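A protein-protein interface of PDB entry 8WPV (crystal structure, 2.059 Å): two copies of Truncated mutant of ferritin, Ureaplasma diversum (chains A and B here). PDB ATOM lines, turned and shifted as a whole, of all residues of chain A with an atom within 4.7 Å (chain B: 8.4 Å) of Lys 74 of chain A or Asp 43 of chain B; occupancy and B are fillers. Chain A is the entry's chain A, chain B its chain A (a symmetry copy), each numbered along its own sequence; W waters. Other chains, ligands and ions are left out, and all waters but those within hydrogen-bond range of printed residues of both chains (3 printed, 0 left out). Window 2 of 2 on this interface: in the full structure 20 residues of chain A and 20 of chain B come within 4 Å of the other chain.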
ATOM      1  N   SER A  70      20.963 -21.049  35.851  1.00  0.00           N
ATOM      2  CA  SER A  70      20.042 -20.325  34.980  1.00  0.00           C
ATOM      3  C   SER A  70      20.273 -20.681  33.517  1.00  0.00           C
ATOM      4  O   SER A  70      19.317 -20.796  32.740  1.00  0.00           O
ATOM      5  CB  SER A  70      20.188 -18.817  35.198  1.00  0.00           C
ATOM      6  OG  SER A  70      19.875 -18.098  34.015  1.00  0.00           O
ATOM      7  N   ASP A  71      21.536 -20.865  33.123  1.00  0.00           N
ATOM      8  CA  ASP A  71      21.829 -21.266  31.750  1.00  0.00           C
ATOM      9  C   ASP A  71      21.380 -22.696  31.480  1.00  0.00           C
ATOM     10  O   ASP A  71      20.830 -22.987  30.412  1.00  0.00           O
ATOM     11  CB  ASP A  71      23.322 -21.110  31.459  1.00  0.00           C
ATOM     12  CG  ASP A  71      23.784 -19.666  31.530  1.00  0.00           C
ATOM     13  OD1 ASP A  71      22.926 -18.760  31.457  1.00  0.00           O
ATOM     14  OD2 ASP A  71      25.006 -19.438  31.649  1.00  0.00           O
ATOM     15  N   TYR A  72      21.613 -23.604  32.433  1.00  0.00           N
ATOM     16  CA  TYR A  72      21.144 -24.977  32.276  1.00  0.00           C
ATOM     17  C   TYR A  72      19.629 -25.024  32.114  1.00  0.00           C
ATOM     18  O   TYR A  72      19.109 -25.802  31.307  1.00  0.00           O
ATOM     19  CB  TYR A  72      21.590 -25.821  33.472  1.00  0.00           C
ATOM     20  CG  TYR A  72      21.158 -27.272  33.417  1.00  0.00           C
ATOM     21  CD1 TYR A  72      21.586 -28.110  32.395  1.00  0.00           C
ATOM     22  CD2 TYR A  72      20.333 -27.806  34.400  1.00  0.00           C
ATOM     23  CE1 TYR A  72      21.196 -29.437  32.347  1.00  0.00           C
ATOM     24  CE2 TYR A  72      19.939 -29.132  34.362  1.00  0.00           C
ATOM     25  CZ  TYR A  72      20.372 -29.943  33.333  1.00  0.00           C
ATOM     26  OH  TYR A  72      19.979 -31.261  33.292  1.00  0.00           O
ATOM     27  N   PHE A  73      18.910 -24.183  32.865  1.00  0.00           N
ATOM     28  CA  PHE A  73      17.455 -24.130  32.746  1.00  0.00           C
ATOM     29  C   PHE A  73      17.027 -23.757  31.331  1.00  0.00           C
ATOM     30  O   PHE A  73      16.053 -24.310  30.805  1.00  0.00           O
ATOM     31  CB  PHE A  73      16.876 -23.133  33.750  1.00  0.00           C
ATOM     32  CG  PHE A  73      16.865 -23.623  35.172  1.00  0.00           C
ATOM     33  CD1 PHE A  73      17.283 -24.905  35.490  1.00  0.00           C
ATOM     34  CD2 PHE A  73      16.419 -22.796  36.193  1.00  0.00           C
ATOM     35  CE1 PHE A  73      17.265 -25.350  36.801  1.00  0.00           C
ATOM     36  CE2 PHE A  73      16.398 -23.235  37.505  1.00  0.00           C
ATOM     37  CZ  PHE A  73      16.819 -24.514  37.809  1.00  0.00           C
ATOM     38  N   LYS A  74      17.742 -22.818  30.702  1.00  0.00           N
ATOM     39  CA  LYS A  74      17.405 -22.408  29.340  1.00  0.00           C
ATOM     40  C   LYS A  74      17.443 -23.582  28.370  1.00  0.00           C
ATOM     41  O   LYS A  74      16.700 -23.597  27.383  1.00  0.00           O
ATOM     42  CB  LYS A  74      18.366 -21.317  28.860  1.00  0.00           C
ATOM     43  CG  LYS A  74      18.240 -19.977  29.571  1.00  0.00           C
ATOM     44  CD  LYS A  74      19.124 -18.929  28.903  1.00  0.00           C
ATOM     45  CE  LYS A  74      19.824 -18.046  29.925  1.00  0.00           C
ATOM     46  NZ  LYS A  74      20.765 -17.093  29.271  1.00  0.00           N
ATOM     47  N   ARG A  75      18.292 -24.574  28.640  1.00  0.00           N
ATOM     48  CA  ARG A  75      18.530 -25.650  27.685  1.00  0.00           C
ATOM     49  C   ARG A  75      17.481 -26.753  27.787  1.00  0.00           C
ATOM     50  O   ARG A  75      17.075 -27.318  26.766  1.00  0.00           O
ATOM     51  CB  ARG A  75      19.929 -26.226  27.905  1.00  0.00           C
ATOM     52  CG  ARG A  75      21.013 -25.164  27.974  1.00  0.00           C
ATOM     53  CD  ARG A  75      22.411 -25.762  27.999  1.00  0.00           C
ATOM     54  NE  ARG A  75      23.394 -24.759  28.397  1.00  0.00           N
ATOM     55  CZ  ARG A  75      24.121 -24.819  29.509  1.00  0.00           C
ATOM     56  NH1 ARG A  75      23.980 -25.840  30.345  1.00  0.00           N
ATOM     57  NH2 ARG A  75      24.989 -23.855  29.788  1.00  0.00           N
ATOM     58  N   ASN A  76      17.031 -27.073  29.000  1.00  0.00           N
ATOM     59  CA  ASN A  76      16.171 -28.229  29.227  1.00  0.00           C
ATOM     60  C   ASN A  76      14.733 -27.854  29.563  1.00  0.00           C
ATOM     61  O   ASN A  76      13.945 -28.732  29.930  1.00  0.00           O
ATOM     62  CB  ASN A  76      16.766 -29.112  30.327  1.00  0.00           C
ATOM     63  CG  ASN A  76      16.784 -28.431  31.684  1.00  0.00           C
ATOM     64  OD1 ASN A  76      16.433 -27.256  31.815  1.00  0.00           O
ATOM     65  ND2 ASN A  76      17.210 -29.167  32.702  1.00  0.00           N
ATOM     66  N   GLY A  77      14.369 -26.579  29.452  1.00  0.00           N
ATOM     67  CA  GLY A  77      12.989 -26.187  29.656  1.00  0.00           C
ATOM     68  C   GLY A  77      12.547 -26.082  31.097  1.00  0.00           C
ATOM     69  O   GLY A  77      11.341 -26.082  31.364  1.00  0.00           O
ATOM     70  N   LYS A  79      12.179 -23.913  34.684  1.00  0.00           N
ATOM     71  CA  LYS A  79      11.858 -22.524  34.979  1.00  0.00           C
ATOM     72  C   LYS A  79      12.714 -22.008  36.126  1.00  0.00           C
ATOM     73  O   LYS A  79      12.970 -22.723  37.100  1.00  0.00           O
ATOM     74  CB  LYS A  79      10.374 -22.364  35.317  1.00  0.00           C
ATOM     75  CG  LYS A  79       9.617 -21.491  34.326  1.00  0.00           C
ATOM     76  CD  LYS A  79      10.007 -21.823  32.890  1.00  0.00           C
ATOM     77  CE  LYS A  79       9.923 -20.599  31.989  1.00  0.00           C
ATOM     78  NZ  LYS A  79      10.457 -20.877  30.627  1.00  0.00           N
ATOM     79  N   ALA B  35      18.960 -10.122  36.605  1.00  0.00           N
ATOM     80  CA  ALA B  35      19.438 -11.458  36.262  1.00  0.00           C
ATOM     81  C   ALA B  35      18.285 -12.354  35.833  1.00  0.00           C
ATOM     82  O   ALA B  35      18.415 -13.136  34.882  1.00  0.00           O
ATOM     83  CB  ALA B  35      20.187 -12.072  37.446  1.00  0.00           C
ATOM     84  N   HIS B  36      17.146 -12.247  36.518  1.00  0.00           N
ATOM     85  CA  HIS B  36      15.954 -12.983  36.109  1.00  0.00           C
ATOM     86  C   HIS B  36      15.434 -12.478  34.769  1.00  0.00           C
ATOM     87  O   HIS B  36      15.127 -13.272  33.871  1.00  0.00           O
ATOM     88  CB  HIS B  36      14.877 -12.862  37.187  1.00  0.00           C
ATOM     89  CG  HIS B  36      13.856 -13.954  37.149  1.00  0.00           C
ATOM     90  ND1 HIS B  36      12.874 -14.021  36.186  1.00  0.00           N
ATOM     91  CD2 HIS B  36      13.659 -15.019  37.961  1.00  0.00           C
ATOM     92  CE1 HIS B  36      12.120 -15.084  36.403  1.00  0.00           C
ATOM     93  NE2 HIS B  36      12.573 -15.705  37.476  1.00  0.00           N
ATOM     94  N   TYR B  37      15.327 -11.153  34.618  1.00  0.00           N
ATOM     95  CA  TYR B  37      14.868 -10.572  33.359  1.00  0.00           C
ATOM     96  C   TYR B  37      15.761 -10.986  32.195  1.00  0.00           C
ATOM     97  O   TYR B  37      15.269 -11.247  31.090  1.00  0.00           O
ATOM     98  CB  TYR B  37      14.827  -9.047  33.466  1.00  0.00           C
ATOM     99  CG  TYR B  37      13.680  -8.486  34.279  1.00  0.00           C
ATOM    100  CD1 TYR B  37      12.736  -9.319  34.869  1.00  0.00           C
ATOM    101  CD2 TYR B  37      13.544  -7.115  34.456  1.00  0.00           C
ATOM    102  CE1 TYR B  37      11.690  -8.799  35.612  1.00  0.00           C
ATOM    103  CE2 TYR B  37      12.502  -6.587  35.193  1.00  0.00           C
ATOM    104  CZ  TYR B  37      11.578  -7.431  35.768  1.00  0.00           C
ATOM    105  OH  TYR B  37      10.543  -6.902  36.503  1.00  0.00           O
ATOM    106  N   ALA B  38      17.078 -11.038  32.418  1.00  0.00           N
ATOM    107  CA  ALA B  38      17.993 -11.461  31.362  1.00  0.00           C
ATOM    108  C   ALA B  38      17.728 -12.902  30.950  1.00  0.00           C
ATOM    109  O   ALA B  38      17.724 -13.226  29.755  1.00  0.00           O
ATOM    110  CB  ALA B  38      19.441 -11.297  31.822  1.00  0.00           C
ATOM    111  N   HIS B  39      17.510 -13.781  31.930  1.00  0.00           N
ATOM    112  CA  HIS B  39      17.161 -15.167  31.635  1.00  0.00           C
ATOM    113  C   HIS B  39      15.881 -15.247  30.812  1.00  0.00           C
ATOM    114  O   HIS B  39      15.792 -16.031  29.860  1.00  0.00           O
ATOM    115  CB  HIS B  39      17.017 -15.947  32.945  1.00  0.00           C
ATOM    116  CG  HIS B  39      16.493 -17.339  32.773  1.00  0.00           C
ATOM    117  ND1 HIS B  39      17.317 -18.428  32.595  1.00  0.00           N
ATOM    118  CD2 HIS B  39      15.227 -17.821  32.765  1.00  0.00           C
ATOM    119  CE1 HIS B  39      16.583 -19.520  32.481  1.00  0.00           C
ATOM    120  NE2 HIS B  39      15.311 -19.179  32.577  1.00  0.00           N
ATOM    121  N   VAL B  40      14.886 -14.428  31.154  1.00  0.00           N
ATOM    122  CA  VAL B  40      13.598 -14.484  30.470  1.00  0.00           C
ATOM    123  C   VAL B  40      13.712 -13.916  29.060  1.00  0.00           C
ATOM    124  O   VAL B  40      13.101 -14.436  28.116  1.00  0.00           O
ATOM    125  CB  VAL B  40      12.534 -13.746  31.303  1.00  0.00           C
ATOM    126  CG1 VAL B  40      11.323 -13.402  30.452  1.00  0.00           C
ATOM    127  CG2 VAL B  40      12.128 -14.590  32.504  1.00  0.00           C
ATOM    128  N   ALA B  41      14.491 -12.843  28.890  1.00  0.00           N
ATOM    129  CA  ALA B  41      14.685 -12.271  27.562  1.00  0.00           C
ATOM    130  C   ALA B  41      15.235 -13.309  26.591  1.00  0.00           C
ATOM    131  O   ALA B  41      14.786 -13.397  25.441  1.00  0.00           O
ATOM    132  CB  ALA B  41      15.620 -11.064  27.643  1.00  0.00           C
ATOM    133  N   ASP B  42      16.198 -14.112  27.042  1.00  0.00           N
ATOM    134  CA  ASP B  42      16.758 -15.159  26.195  1.00  0.00           C
ATOM    135  C   ASP B  42      15.775 -16.312  26.031  1.00  0.00           C
ATOM    136  O   ASP B  42      15.419 -16.688  24.908  1.00  0.00           O
ATOM    137  CB  ASP B  42      18.082 -15.650  26.787  1.00  0.00           C
ATOM    138  CG  ASP B  42      18.821 -16.609  25.866  1.00  0.00           C
ATOM    139  OD1 ASP B  42      18.345 -16.861  24.738  1.00  0.00           O
ATOM    140  OD2 ASP B  42      19.889 -17.114  26.276  1.00  0.00           O
ATOM    141  N   ASP B  43      15.311 -16.877  27.147  1.00  0.00           N
ATOM    142  CA  ASP B  43      14.591 -18.143  27.087  1.00  0.00           C
ATOM    143  C   ASP B  43      13.173 -17.976  26.549  1.00  0.00           C
ATOM    144  O   ASP B  43      12.768 -18.694  25.629  1.00  0.00           O
ATOM    145  CB  ASP B  43      14.567 -18.799  28.469  1.00  0.00           C
ATOM    146  CG  ASP B  43      14.008 -20.207  28.431  1.00  0.00           C
ATOM    147  OD1 ASP B  43      14.563 -21.049  27.692  1.00  0.00           O
ATOM    148  OD2 ASP B  43      13.014 -20.470  29.137  1.00  0.00           O
ATOM    149  N   GLU B  44      12.400 -17.045  27.112  1.00  0.00           N
ATOM    150  CA  GLU B  44      11.005 -16.930  26.697  1.00  0.00           C
ATOM    151  C   GLU B  44      10.829 -16.057  25.461  1.00  0.00           C
ATOM    152  O   GLU B  44       9.919 -16.305  24.663  1.00  0.00           O
ATOM    153  CB  GLU B  44      10.145 -16.378  27.836  1.00  0.00           C
ATOM    154  CG  GLU B  44       8.668 -16.732  27.685  1.00  0.00           C
ATOM    155  CD  GLU B  44       7.744 -15.784  28.424  1.00  0.00           C
ATOM    156  OE1 GLU B  44       8.147 -15.254  29.481  1.00  0.00           O
ATOM    157  OE2 GLU B  44       6.609 -15.568  27.945  1.00  0.00           O
ATOM    158  N   PHE B  45      11.672 -15.042  25.277  1.00  0.00           N
ATOM    159  CA  PHE B  45      11.451 -14.058  24.229  1.00  0.00           C
ATOM    160  C   PHE B  45      12.388 -14.200  23.038  1.00  0.00           C
ATOM    161  O   PHE B  45      12.260 -13.427  22.082  1.00  0.00           O
ATOM    162  CB  PHE B  45      11.563 -12.639  24.808  1.00  0.00           C
ATOM    163  CG  PHE B  45      10.510 -12.327  25.841  1.00  0.00           C
ATOM    164  CD1 PHE B  45       9.251 -12.901  25.755  1.00  0.00           C
ATOM    165  CD2 PHE B  45      10.779 -11.472  26.897  1.00  0.00           C
ATOM    166  CE1 PHE B  45       8.279 -12.626  26.702  1.00  0.00           C
ATOM    167  CE2 PHE B  45       9.811 -11.192  27.847  1.00  0.00           C
ATOM    168  CZ  PHE B  45       8.560 -11.772  27.750  1.00  0.00           C
ATOM    169  N   ASP B  46      13.319 -15.157  23.065  1.00  0.00           N
ATOM    170  CA  ASP B  46      14.199 -15.455  21.934  1.00  0.00           C
ATOM    171  C   ASP B  46      15.097 -14.279  21.565  1.00  0.00           C
ATOM    172  O   ASP B  46      15.427 -14.092  20.393  1.00  0.00           O
ATOM    173  CB  ASP B  46      13.395 -15.898  20.708  1.00  0.00           C
ATOM    174  CG  ASP B  46      12.353 -16.931  21.048  1.00  0.00           C
ATOM    175  OD1 ASP B  46      12.440 -17.509  22.150  1.00  0.00           O
ATOM    176  OD2 ASP B  46      11.439 -17.158  20.228  1.00  0.00           O
ATOM    177  N   MET B  47      15.510 -13.480  22.547  1.00  0.00           N
ATOM    178  CA  MET B  47      16.370 -12.323  22.310  1.00  0.00           C
ATOM    179  C   MET B  47      17.624 -12.439  23.167  1.00  0.00           C
ATOM    180  O   MET B  47      17.790 -11.704  24.154  1.00  0.00           O
ATOM    181  CB  MET B  47      15.623 -11.020  22.581  1.00  0.00           C
ATOM    182  CG  MET B  47      14.381 -10.863  21.716  1.00  0.00           C
ATOM    183  SD  MET B  47      13.633  -9.227  21.784  1.00  0.00           S
ATOM    184  CE  MET B  47      14.843  -8.239  20.904  1.00  0.00           C
ATOM    185  N   PRO B  48      18.540 -13.346  22.812  1.00  0.00           N
ATOM    186  CA  PRO B  48      19.723 -13.567  23.658  1.00  0.00           C
ATOM    187  C   PRO B  48      20.618 -12.349  23.798  1.00  0.00           C
ATOM    188  O   PRO B  48      21.317 -12.223  24.810  1.00  0.00           O
ATOM    189  CB  PRO B  48      20.449 -14.721  22.950  1.00  0.00           C
ATOM    190  CG  PRO B  48      19.910 -14.720  21.550  1.00  0.00           C
ATOM    191  CD  PRO B  48      18.491 -14.281  21.676  1.00  0.00           C
ATOM    192  N   GLY B  51      19.119 -10.285  26.322  1.00  0.00           N
ATOM    193  CA  GLY B  51      19.462 -10.908  27.590  1.00  0.00           C
ATOM    194  C   GLY B  51      20.861 -10.548  28.053  1.00  0.00           C
ATOM    195  O   GLY B  51      21.076 -10.222  29.224  1.00  0.00           O
ATOM    196  N   LYS B  52      21.833 -10.600  27.139  1.00  0.00           N
ATOM    197  CA  LYS B  52      23.194 -10.230  27.513  1.00  0.00           C
ATOM    198  C   LYS B  52      23.291  -8.761  27.900  1.00  0.00           C
ATOM    199  O   LYS B  52      24.068  -8.411  28.797  1.00  0.00           O
ATOM    200  CB  LYS B  52      24.170 -10.554  26.381  1.00  0.00           C
ATOM    201  CG  LYS B  52      24.230 -12.033  26.038  1.00  0.00           C
ATOM    202  CD  LYS B  52      25.571 -12.418  25.439  1.00  0.00           C
ATOM    203  CE  LYS B  52      25.432 -12.746  23.964  1.00  0.00           C
ATOM    204  NZ  LYS B  52      25.519 -14.212  23.714  1.00  0.00           N
ATOM    205  N   GLN B  55      21.851  -8.723  31.352  1.00  0.00           N
ATOM    206  CA  GLN B  55      22.763  -9.425  32.251  1.00  0.00           C
ATOM    207  C   GLN B  55      23.952  -8.550  32.629  1.00  0.00           C
ATOM    208  O   GLN B  55      24.434  -8.602  33.767  1.00  0.00           O
ATOM    209  CB  GLN B  55      23.234 -10.730  31.607  1.00  0.00           C
ATOM    210  CG  GLN B  55      24.198 -11.547  32.458  1.00  0.00           C
ATOM    211  CD  GLN B  55      23.609 -11.960  33.796  1.00  0.00           C
ATOM    212  OE1 GLN B  55      22.429 -12.296  33.892  1.00  0.00           O
ATOM    213  NE2 GLN B  55      24.434 -11.941  34.838  1.00  0.00           N
HETATM  214  O   HOH W   1      12.099 -18.259  30.531  1.00  0.00           O
HETATM  215  O   HOH W   2      20.685 -15.045  31.303  1.00  0.00           O
HETATM  216  O   HOH W   3      20.538 -14.739  34.025  1.00  0.00           O
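A ring nitrogen (ND1) of His 39 of chain B is in hydrogen-bond range of the side-chain hydroxyl (OG) of Ser 70 of chain A.
The side-chain amino group of Lys 74 of chain A is in salt-bridge range of the side-chain carboxylate of Asp 42 of chain B (3.1 Å).
The side-chain amino group (NZ) of Lys 79 of chain A is in salt-bridge range of the side-chain carboxylate (OD2) of Asp 43 of chain B, 3.0 Å away.
The backbone carbonyl oxygen (O) of Lys 74 of chain A sits close to the side-chain carboxylate (OD1) of Asp 43 of chain B (3.3 Å).
NZ of Lys 74 of chain A lies within salt-bridge range of OD1 of Asp 71 of chain A (3.5 Å).
The backbone carbonyl oxygen (O) of Phe 73 of chain A lies close to the side-chain amide oxygen (OD1) of Asn 76 of chain A (3.1 Å).
His 39 of chain B touches Phe 73 of chain A.
CG of Lys 74 of chain A touches CE1 of His 39 of chain B, at 3.4 Å.
Of chain A, only Lys 74 (3.3 Å) and Lys 79 (3.0 Å) come within 4 Å of Asp 43 of chain B.
Printed residues of chain A within 4 Å of His 39 of chain B: Ser 70, Phe 73 and Lys 74.
Of the printed residues of chain A, Asp 42 of chain B touches Lys 74.
Of the printed residues of chain B, Ser 70 of chain A touches His 39.
Printed residues of chain B within 4 Å of Lys 79 of chain A: Asp 43 (3.0 Å).
Ala 38 of chain B touches none of the printed residues of chain A.
Asp 46 of chain B touches none of the printed residues of chain A.
The nearest printed residue of chain B that does not touch Phe 73 of chain A is Asp 43 of chain B (4.7 Å).
Hydrophobic or aromatic side chains of chain B that line the printed part of chain A: His 39.
Of the 9 printed residues of chain A, 4 touch a printed residue of chain B.
Hydrophobic or aromatic side chains of chain A that line the printed part of chain B: Phe 73.
No position is printed for both chains.
Water W1 bridges OD2 of Asp 43 of chain B (2.8 Å) and NZ of Lys 79 of chain A (3.1 Å).
Water W3 lies within hydrogen-bond range of O of Ala 35 of chain B (2.8 Å), OE1 of Gln 55 of chain B (3.1 Å) and OG of Ser 70 of chain A (3.4 Å).
Water W2 bridges NZ of Lys 74 of chain A (2.9 Å) and N of His 39 of chain B (3.5 Å).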
